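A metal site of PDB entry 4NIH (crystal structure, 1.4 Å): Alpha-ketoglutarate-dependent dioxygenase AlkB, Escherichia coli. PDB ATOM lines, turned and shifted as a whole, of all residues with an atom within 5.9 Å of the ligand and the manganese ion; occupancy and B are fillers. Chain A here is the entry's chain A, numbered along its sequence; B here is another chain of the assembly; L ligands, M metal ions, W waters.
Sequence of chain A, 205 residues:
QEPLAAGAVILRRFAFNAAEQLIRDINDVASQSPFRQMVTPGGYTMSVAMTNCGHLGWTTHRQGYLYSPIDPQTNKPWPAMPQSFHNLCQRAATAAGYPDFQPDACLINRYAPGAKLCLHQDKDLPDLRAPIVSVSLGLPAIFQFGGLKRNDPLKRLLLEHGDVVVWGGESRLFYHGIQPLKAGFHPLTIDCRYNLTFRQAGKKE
The manganese ion is bound by OD1 of Asp 122 (2.1 Å), O1 of the ligand (2.2 Å), NE2 of His 176 (2.2 Å), NE2 of His 120 (2.3 Å), O3 of the ligand (2.3 Å) and water W2 (2.3 Å).
A ring nitrogen (ND1) of His 120 is in hydrogen-bond range of O4' of 6MA 8 of chain B (3.4 Å). The backbone carbonyl oxygen of Arg 193 lies within hydrogen-bond range of the backbone NH of Tyr 111, 2.8 Å away. O of Asn 195 is in hydrogen-bond range of N of Asn 109, 2.9 Å away. The side-chain sulfur of Met 50 sits close to the side-chain amide nitrogen of Asn 109 (3.8 Å). The side-chain amide nitrogen of Asn 195 lies close to the guanidinium group of Arg 193 (3.2 Å). NH2 of Arg 193 sits at hydrogen-bond distance from OG of Ser 136 (2.9 Å). The side-chain amide oxygen (OD1) of Asn 195 lies within hydrogen-bond range of the side-chain hydroxyl (OG1) of Thr 197 (3.1 Å). OD1 of Asn 195 sits at hydrogen-bond distance from OG of Ser 134 (3.0 Å).
Water W4 lies within hydrogen-bond range of N1 of 6MA 8 of chain B and OD2 of Asp 122. Water W1 bridges the side-chain hydroxyl (OG) of Ser 134 and an oxygen (O4) of the ligand. Water W3 bridges the side-chain hydroxyl of Thr 197 and the side-chain hydroxyl of Ser 134.
The side-chain hydroxyl (OH) of Tyr 111 is in hydrogen-bond range of an oxygen (O5) of the ligand. The side-chain amide oxygen of Asn 109 sits close to an oxygen (O2) of the ligand (2.8 Å). O5 of the ligand lies within salt-bridge range of NH1 of Arg 193. O4 of the ligand lies within hydrogen-bond range of ND2 of Asn 195 (3.3 Å).
Within 4 Å of the manganese ion: His 120, Asp 122 and His 176.
An oxygen (O1) of the ligand sits close to N1 of 6MA 8 of chain B, at 3.4 Å. Leu 107 touches the ligand. CD2 of Leu 117 touches C2 of the ligand (3.5 Å). OG of Ser 134 touches O4 of the ligand, 3.98 Å away. CD1 of Ile 178 touches O4 of the ligand, 3.4 Å away. Thr 197 touches the ligand. Hydrophobic or aromatic side chains within 4 Å of the ligand: Leu 107, Tyr 111, Leu 117, His 120, His 176 and Ile 178. The nearest printed residue that does not touch the ligand is Leu 159 (4.1 Å).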
ATOM      1  N   MET A  50     -27.810  -9.229 -33.893  1.00  0.00           N
ATOM      2  CA  MET A  50     -27.616  -8.584 -32.600  1.00  0.00           C
ATOM      3  C   MET A  50     -27.798  -7.086 -32.620  1.00  0.00           C
ATOM      4  O   MET A  50     -27.594  -6.423 -33.642  1.00  0.00           O
ATOM      5  CB  MET A  50     -26.199  -8.880 -32.132  1.00  0.00           C
ATOM      6  CG  MET A  50     -25.962 -10.339 -31.742  1.00  0.00           C
ATOM      7  SD  MET A  50     -24.242 -10.766 -31.402  1.00  0.00           S
ATOM      8  CE  MET A  50     -24.340 -12.299 -30.466  1.00  0.00           C
ATOM      9  N   LEU A 107     -26.927  -7.034 -24.400  1.00  0.00           N
ATOM     10  CA  LEU A 107     -26.820  -7.577 -25.732  1.00  0.00           C
ATOM     11  C   LEU A 107     -28.136  -8.259 -26.082  1.00  0.00           C
ATOM     12  O   LEU A 107     -28.571  -9.130 -25.326  1.00  0.00           O
ATOM     13  CB  LEU A 107     -25.656  -8.562 -25.821  1.00  0.00           C
ATOM     14  CG  LEU A 107     -25.510  -9.400 -27.092  1.00  0.00           C
ATOM     15  CD1 LEU A 107     -25.285  -8.516 -28.296  1.00  0.00           C
ATOM     16  CD2 LEU A 107     -24.370 -10.390 -26.893  1.00  0.00           C
ATOM     17  N   ASN A 109     -30.178 -10.445 -28.724  1.00  0.00           N
ATOM     18  CA  ASN A 109     -30.006 -11.431 -29.777  1.00  0.00           C
ATOM     19  C   ASN A 109     -31.345 -11.746 -30.419  1.00  0.00           C
ATOM     20  O   ASN A 109     -32.358 -11.802 -29.718  1.00  0.00           O
ATOM     21  CB  ASN A 109     -29.421 -12.717 -29.163  1.00  0.00           C
ATOM     22  CG  ASN A 109     -28.030 -12.507 -28.575  1.00  0.00           C
ATOM     23  OD1 ASN A 109     -27.766 -12.811 -27.411  1.00  0.00           O
ATOM     24  ND2 ASN A 109     -27.169 -11.967 -29.360  1.00  0.00           N
ATOM     25  N   TYR A 111     -32.883 -14.670 -32.992  1.00  0.00           N
ATOM     26  CA  TYR A 111     -32.697 -15.940 -33.680  1.00  0.00           C
ATOM     27  C   TYR A 111     -33.852 -16.202 -34.631  1.00  0.00           C
ATOM     28  O   TYR A 111     -35.009 -16.330 -34.198  1.00  0.00           O
ATOM     29  CB  TYR A 111     -32.651 -17.097 -32.664  1.00  0.00           C
ATOM     30  CG  TYR A 111     -31.543 -17.031 -31.652  1.00  0.00           C
ATOM     31  CD1 TYR A 111     -31.612 -16.189 -30.553  1.00  0.00           C
ATOM     32  CD2 TYR A 111     -30.420 -17.850 -31.791  1.00  0.00           C
ATOM     33  CE1 TYR A 111     -30.576 -16.149 -29.627  1.00  0.00           C
ATOM     34  CE2 TYR A 111     -29.375 -17.813 -30.863  1.00  0.00           C
ATOM     35  CZ  TYR A 111     -29.473 -16.961 -29.798  1.00  0.00           C
ATOM     36  OH  TYR A 111     -28.440 -16.914 -28.888  1.00  0.00           O
ATOM     37  N   LEU A 117     -25.780 -20.275 -31.712  1.00  0.00           N
ATOM     38  CA  LEU A 117     -24.615 -19.615 -31.090  1.00  0.00           C
ATOM     39  C   LEU A 117     -23.712 -20.696 -30.556  1.00  0.00           C
ATOM     40  O   LEU A 117     -24.013 -21.356 -29.562  1.00  0.00           O
ATOM     41  CB  LEU A 117     -25.073 -18.655 -29.993  1.00  0.00           C
ATOM     42  CG  LEU A 117     -24.128 -17.555 -29.591  1.00  0.00           C
ATOM     43  CD1 LEU A 117     -23.699 -16.719 -30.785  1.00  0.00           C
ATOM     44  CD2 LEU A 117     -24.771 -16.699 -28.501  1.00  0.00           C
ATOM     45  N   HIS A 120     -19.319 -21.005 -26.289  1.00  0.00           N
ATOM     46  CA  HIS A 120     -18.350 -19.970 -26.021  1.00  0.00           C
ATOM     47  C   HIS A 120     -18.394 -19.651 -24.529  1.00  0.00           C
ATOM     48  O   HIS A 120     -19.273 -20.112 -23.794  1.00  0.00           O
ATOM     49  CB  HIS A 120     -18.688 -18.707 -26.838  1.00  0.00           C
ATOM     50  CG  HIS A 120     -19.992 -18.101 -26.464  1.00  0.00           C
ATOM     51  ND1 HIS A 120     -21.188 -18.551 -26.961  1.00  0.00           N
ATOM     52  CD2 HIS A 120     -20.290 -17.077 -25.632  1.00  0.00           C
ATOM     53  CE1 HIS A 120     -22.177 -17.823 -26.451  1.00  0.00           C
ATOM     54  NE2 HIS A 120     -21.656 -16.932 -25.637  1.00  0.00           N
ATOM     55  N   GLN A 121     -17.432 -18.847 -24.094  1.00  0.00           N
ATOM     56  CA  GLN A 121     -17.390 -18.295 -22.746  1.00  0.00           C
ATOM     57  C   GLN A 121     -17.646 -16.804 -22.863  1.00  0.00           C
ATOM     58  O   GLN A 121     -17.192 -16.160 -23.807  1.00  0.00           O
ATOM     59  CB  GLN A 121     -16.018 -18.535 -22.124  1.00  0.00           C
ATOM     60  CG  GLN A 121     -15.589 -19.989 -22.009  1.00  0.00           C
ATOM     61  CD  GLN A 121     -14.146 -20.099 -21.525  1.00  0.00           C
ATOM     62  OE1 GLN A 121     -13.208 -19.931 -22.306  1.00  0.00           O
ATOM     63  NE2 GLN A 121     -13.964 -20.335 -20.245  1.00  0.00           N
ATOM     64  N   ASP A 122     -18.376 -16.250 -21.900  1.00  0.00           N
ATOM     65  CA  ASP A 122     -18.417 -14.803 -21.689  1.00  0.00           C
ATOM     66  C   ASP A 122     -17.242 -14.503 -20.738  1.00  0.00           C
ATOM     67  O   ASP A 122     -17.336 -14.720 -19.531  1.00  0.00           O
ATOM     68  CB  ASP A 122     -19.749 -14.350 -21.076  1.00  0.00           C
ATOM     69  CG  ASP A 122     -20.915 -14.282 -22.084  1.00  0.00           C
ATOM     70  OD1 ASP A 122     -21.044 -15.145 -22.993  1.00  0.00           O
ATOM     71  OD2 ASP A 122     -21.739 -13.331 -21.930  1.00  0.00           O
ATOM     72  N   ILE A 132     -24.098 -12.804 -15.089  1.00  0.00           N
ATOM     73  CA  ILE A 132     -24.814 -12.700 -16.337  1.00  0.00           C
ATOM     74  C   ILE A 132     -26.280 -13.034 -16.082  1.00  0.00           C
ATOM     75  O   ILE A 132     -26.573 -14.049 -15.471  1.00  0.00           O
ATOM     76  CB  ILE A 132     -24.267 -13.664 -17.385  1.00  0.00           C
ATOM     77  CG1 ILE A 132     -22.816 -13.295 -17.751  1.00  0.00           C
ATOM     78  CG2 ILE A 132     -25.145 -13.661 -18.645  1.00  0.00           C
ATOM     79  CD1 ILE A 132     -22.025 -14.435 -18.338  1.00  0.00           C
ATOM     80  N   SER A 134     -29.759 -13.647 -18.304  1.00  0.00           N
ATOM     81  CA  SER A 134     -30.007 -14.014 -19.689  1.00  0.00           C
ATOM     82  C   SER A 134     -31.482 -14.348 -19.841  1.00  0.00           C
ATOM     83  O   SER A 134     -31.954 -15.328 -19.284  1.00  0.00           O
ATOM     84  CB  SER A 134     -29.127 -15.213 -20.056  1.00  0.00           C
ATOM     85  OG  SER A 134     -29.146 -15.497 -21.447  1.00  0.00           O
ATOM     86  N   SER A 136     -34.990 -15.129 -22.032  1.00  0.00           N
ATOM     87  CA  SER A 136     -35.512 -15.727 -23.268  1.00  0.00           C
ATOM     88  C   SER A 136     -36.907 -15.204 -23.570  1.00  0.00           C
ATOM     89  O   SER A 136     -37.763 -15.104 -22.669  1.00  0.00           O
ATOM     90  CB  SER A 136     -35.646 -17.247 -23.124  1.00  0.00           C
ATOM     91  OG  SER A 136     -34.404 -17.894 -22.956  1.00  0.00           O
ATOM     92  N   PHE A 143     -30.544 -24.668 -24.998  1.00  0.00           N
ATOM     93  CA  PHE A 143     -29.399 -24.016 -24.389  1.00  0.00           C
ATOM     94  C   PHE A 143     -28.436 -25.086 -23.888  1.00  0.00           C
ATOM     95  O   PHE A 143     -28.855 -26.023 -23.212  1.00  0.00           O
ATOM     96  CB  PHE A 143     -29.903 -23.153 -23.229  1.00  0.00           C
ATOM     97  CG  PHE A 143     -28.836 -22.368 -22.475  1.00  0.00           C
ATOM     98  CD1 PHE A 143     -28.149 -21.364 -23.095  1.00  0.00           C
ATOM     99  CD2 PHE A 143     -28.606 -22.595 -21.117  1.00  0.00           C
ATOM    100  CE1 PHE A 143     -27.205 -20.632 -22.397  1.00  0.00           C
ATOM    101  CE2 PHE A 143     -27.682 -21.842 -20.412  1.00  0.00           C
ATOM    102  CZ  PHE A 143     -26.978 -20.864 -21.061  1.00  0.00           C
ATOM    103  N   LEU A 159     -35.105 -23.659 -23.241  1.00  0.00           N
ATOM    104  CA  LEU A 159     -35.473 -22.358 -22.719  1.00  0.00           C
ATOM    105  C   LEU A 159     -36.714 -21.864 -23.472  1.00  0.00           C
ATOM    106  O   LEU A 159     -36.718 -21.778 -24.706  1.00  0.00           O
ATOM    107  CB  LEU A 159     -34.327 -21.367 -22.856  1.00  0.00           C
ATOM    108  CG  LEU A 159     -33.013 -21.712 -22.146  1.00  0.00           C
ATOM    109  CD1 LEU A 159     -32.027 -20.561 -22.309  1.00  0.00           C
ATOM    110  CD2 LEU A 159     -33.182 -22.072 -20.684  1.00  0.00           C
ATOM    111  N   TRP A 167     -25.922 -16.779 -14.240  1.00  0.00           N
ATOM    112  CA  TRP A 167     -24.697 -17.456 -13.816  1.00  0.00           C
ATOM    113  C   TRP A 167     -23.636 -16.461 -13.438  1.00  0.00           C
ATOM    114  O   TRP A 167     -23.675 -15.298 -13.834  1.00  0.00           O
ATOM    115  CB  TRP A 167     -24.218 -18.533 -14.811  1.00  0.00           C
ATOM    116  CG  TRP A 167     -23.786 -18.127 -16.187  1.00  0.00           C
ATOM    117  CD1 TRP A 167     -22.500 -18.068 -16.654  1.00  0.00           C
ATOM    118  CD2 TRP A 167     -24.627 -17.863 -17.326  1.00  0.00           C
ATOM    119  NE1 TRP A 167     -22.495 -17.727 -17.985  1.00  0.00           N
ATOM    120  CE2 TRP A 167     -23.788 -17.612 -18.430  1.00  0.00           C
ATOM    121  CE3 TRP A 167     -26.014 -17.815 -17.508  1.00  0.00           C
ATOM    122  CZ2 TRP A 167     -24.298 -17.309 -19.696  1.00  0.00           C
ATOM    123  CZ3 TRP A 167     -26.513 -17.519 -18.779  1.00  0.00           C
ATOM    124  CH2 TRP A 167     -25.654 -17.276 -19.852  1.00  0.00           C
ATOM    125  N   HIS A 176     -21.122 -22.177 -22.898  1.00  0.00           N
ATOM    126  CA  HIS A 176     -22.559 -22.284 -23.128  1.00  0.00           C
ATOM    127  C   HIS A 176     -22.852 -21.881 -24.558  1.00  0.00           C
ATOM    128  O   HIS A 176     -22.017 -21.285 -25.240  1.00  0.00           O
ATOM    129  CB  HIS A 176     -23.310 -21.370 -22.149  1.00  0.00           C
ATOM    130  CG  HIS A 176     -22.908 -19.942 -22.279  1.00  0.00           C
ATOM    131  ND1 HIS A 176     -21.759 -19.454 -21.722  1.00  0.00           N
ATOM    132  CD2 HIS A 176     -23.450 -18.917 -22.992  1.00  0.00           C
ATOM    133  CE1 HIS A 176     -21.614 -18.191 -22.054  1.00  0.00           C
ATOM    134  NE2 HIS A 176     -22.619 -17.844 -22.825  1.00  0.00           N
ATOM    135  N   GLY A 177     -24.048 -22.217 -25.014  1.00  0.00           N
ATOM    136  CA  GLY A 177     -24.464 -21.846 -26.341  1.00  0.00           C
ATOM    137  C   GLY A 177     -25.888 -22.220 -26.653  1.00  0.00           C
ATOM    138  O   GLY A 177     -26.621 -22.662 -25.774  1.00  0.00           O
ATOM    139  N   ILE A 178     -26.299 -22.025 -27.901  1.00  0.00           N
ATOM    140  CA  ILE A 178     -27.659 -22.284 -28.369  1.00  0.00           C
ATOM    141  C   ILE A 178     -27.603 -23.134 -29.638  1.00  0.00           C
ATOM    142  O   ILE A 178     -26.896 -22.815 -30.583  1.00  0.00           O
ATOM    143  CB  ILE A 178     -28.417 -20.955 -28.645  1.00  0.00           C
ATOM    144  CG1 ILE A 178     -28.690 -20.197 -27.351  1.00  0.00           C
ATOM    145  CG2 ILE A 178     -29.720 -21.181 -29.416  1.00  0.00           C
ATOM    146  CD1 ILE A 178     -29.816 -20.717 -26.491  1.00  0.00           C
ATOM    147  N   ARG A 193     -36.934 -15.971 -31.884  1.00  0.00           N
ATOM    148  CA  ARG A 193     -36.588 -15.929 -30.465  1.00  0.00           C
ATOM    149  C   ARG A 193     -35.704 -14.722 -30.240  1.00  0.00           C
ATOM    150  O   ARG A 193     -34.832 -14.431 -31.060  1.00  0.00           O
ATOM    151  CB  ARG A 193     -35.841 -17.202 -30.037  1.00  0.00           C
ATOM    152  CG  ARG A 193     -35.323 -17.164 -28.614  1.00  0.00           C
ATOM    153  CD  ARG A 193     -34.613 -18.455 -28.245  1.00  0.00           C
ATOM    154  NE  ARG A 193     -34.144 -18.459 -26.862  1.00  0.00           N
ATOM    155  CZ  ARG A 193     -32.909 -18.144 -26.463  1.00  0.00           C
ATOM    156  NH1 ARG A 193     -31.958 -17.847 -27.343  1.00  0.00           N
ATOM    157  NH2 ARG A 193     -32.625 -18.157 -25.173  1.00  0.00           N
ATOM    158  N   ASN A 195     -33.188 -12.984 -27.134  1.00  0.00           N
ATOM    159  CA  ASN A 195     -32.526 -13.140 -25.833  1.00  0.00           C
ATOM    160  C   ASN A 195     -31.966 -11.784 -25.414  1.00  0.00           C
ATOM    161  O   ASN A 195     -31.527 -11.016 -26.271  1.00  0.00           O
ATOM    162  CB  ASN A 195     -31.419 -14.202 -25.848  1.00  0.00           C
ATOM    163  CG  ASN A 195     -30.967 -14.597 -24.456  1.00  0.00           C
ATOM    164  OD1 ASN A 195     -29.906 -14.164 -23.989  1.00  0.00           O
ATOM    165  ND2 ASN A 195     -31.780 -15.380 -23.776  1.00  0.00           N
ATOM    166  N   THR A 197     -29.099 -10.327 -22.797  1.00  0.00           N
ATOM    167  CA  THR A 197     -27.926 -10.700 -21.991  1.00  0.00           C
ATOM    168  C   THR A 197     -27.395  -9.472 -21.288  1.00  0.00           C
ATOM    169  O   THR A 197     -26.825  -8.590 -21.932  1.00  0.00           O
ATOM    170  CB  THR A 197     -26.833 -11.345 -22.868  1.00  0.00           C
ATOM    171  OG1 THR A 197     -27.343 -12.565 -23.423  1.00  0.00           O
ATOM    172  CG2 THR A 197     -25.559 -11.639 -22.080  1.00  0.00           C
ATOM    173  P   6MA B   8     -15.746 -18.377 -29.824  1.00  0.00           P
ATOM    174  OP1 6MA B   8     -15.998 -19.242 -28.625  1.00  0.00           O
ATOM    175  OP2 6MA B   8     -15.123 -17.034 -29.608  1.00  0.00           O
ATOM    176  O5' 6MA B   8     -17.093 -18.139 -30.687  1.00  0.00           O
ATOM    177  C5' 6MA B   8     -18.153 -19.067 -30.767  1.00  0.00           C
ATOM    178  C4' 6MA B   8     -19.441 -18.316 -31.039  1.00  0.00           C
ATOM    179  O4' 6MA B   8     -19.788 -17.532 -29.879  1.00  0.00           O
ATOM    180  C3' 6MA B   8     -19.346 -17.371 -32.237  1.00  0.00           C
ATOM    181  O3' 6MA B   8     -20.568 -17.178 -32.967  1.00  0.00           O
ATOM    182  C2' 6MA B   8     -19.089 -16.027 -31.549  1.00  0.00           C
ATOM    183  C1' 6MA B   8     -19.857 -16.157 -30.241  1.00  0.00           C
ATOM    184  N9  6MA B   8     -19.306 -15.430 -29.088  1.00  0.00           N
ATOM    185  C8  6MA B   8     -18.041 -15.542 -28.596  1.00  0.00           C
ATOM    186  N7  6MA B   8     -17.901 -14.817 -27.488  1.00  0.00           N
ATOM    187  C5  6MA B   8     -19.064 -14.208 -27.223  1.00  0.00           C
ATOM    188  C6  6MA B   8     -19.560 -13.292 -26.196  1.00  0.00           C
ATOM    189  N1  6MA B   8     -20.859 -12.927 -26.301  1.00  0.00           N
ATOM    190  C2  6MA B   8     -21.666 -13.362 -27.294  1.00  0.00           C
ATOM    191  N3  6MA B   8     -21.285 -14.175 -28.273  1.00  0.00           N
ATOM    192  C4  6MA B   8     -20.003 -14.635 -28.267  1.00  0.00           C
ATOM    193  N6  6MA B   8     -18.744 -12.844 -25.219  1.00  0.00           N
ATOM    194  C1  6MA B   8     -19.176 -11.849 -24.254  1.00  0.00           C
HETATM  195  C1  LIG L   1     -24.804 -14.512 -25.558  1.00  0.00           C
HETATM  196  O1  LIG L   1     -23.633 -14.351 -25.054  1.00  0.00           O
HETATM  197  O2  LIG L   1     -25.375 -13.665 -26.302  1.00  0.00           O
HETATM  198  C2  LIG L   1     -25.488 -15.779 -25.250  1.00  0.00           C
HETATM  199  O3  LIG L   1     -24.794 -16.672 -24.711  1.00  0.00           O
HETATM  200  C3  LIG L   1     -26.949 -15.949 -25.628  1.00  0.00           C
HETATM  201  C4  LIG L   1     -27.631 -17.126 -24.953  1.00  0.00           C
HETATM  202  C5  LIG L   1     -29.088 -17.288 -25.367  1.00  0.00           C
HETATM  203  O4  LIG L   1     -29.835 -17.874 -24.564  1.00  0.00           O
HETATM  204  O5  LIG L   1     -29.478 -16.804 -26.465  1.00  0.00           O
HETATM  205 MN    MN M   1     -22.750 -15.960 -23.923  1.00  0.00          MN
HETATM  206  O   HOH W   1     -29.616 -18.109 -21.888  1.00  0.00           O
HETATM  207  O   HOH W   2     -23.918 -15.066 -22.093  1.00  0.00           O
HETATM  208  O   HOH W   3     -26.543 -14.934 -22.421  1.00  0.00           O
HETATM  209  O   HOH W   4     -22.562 -12.044 -24.279  1.00  0.00           O
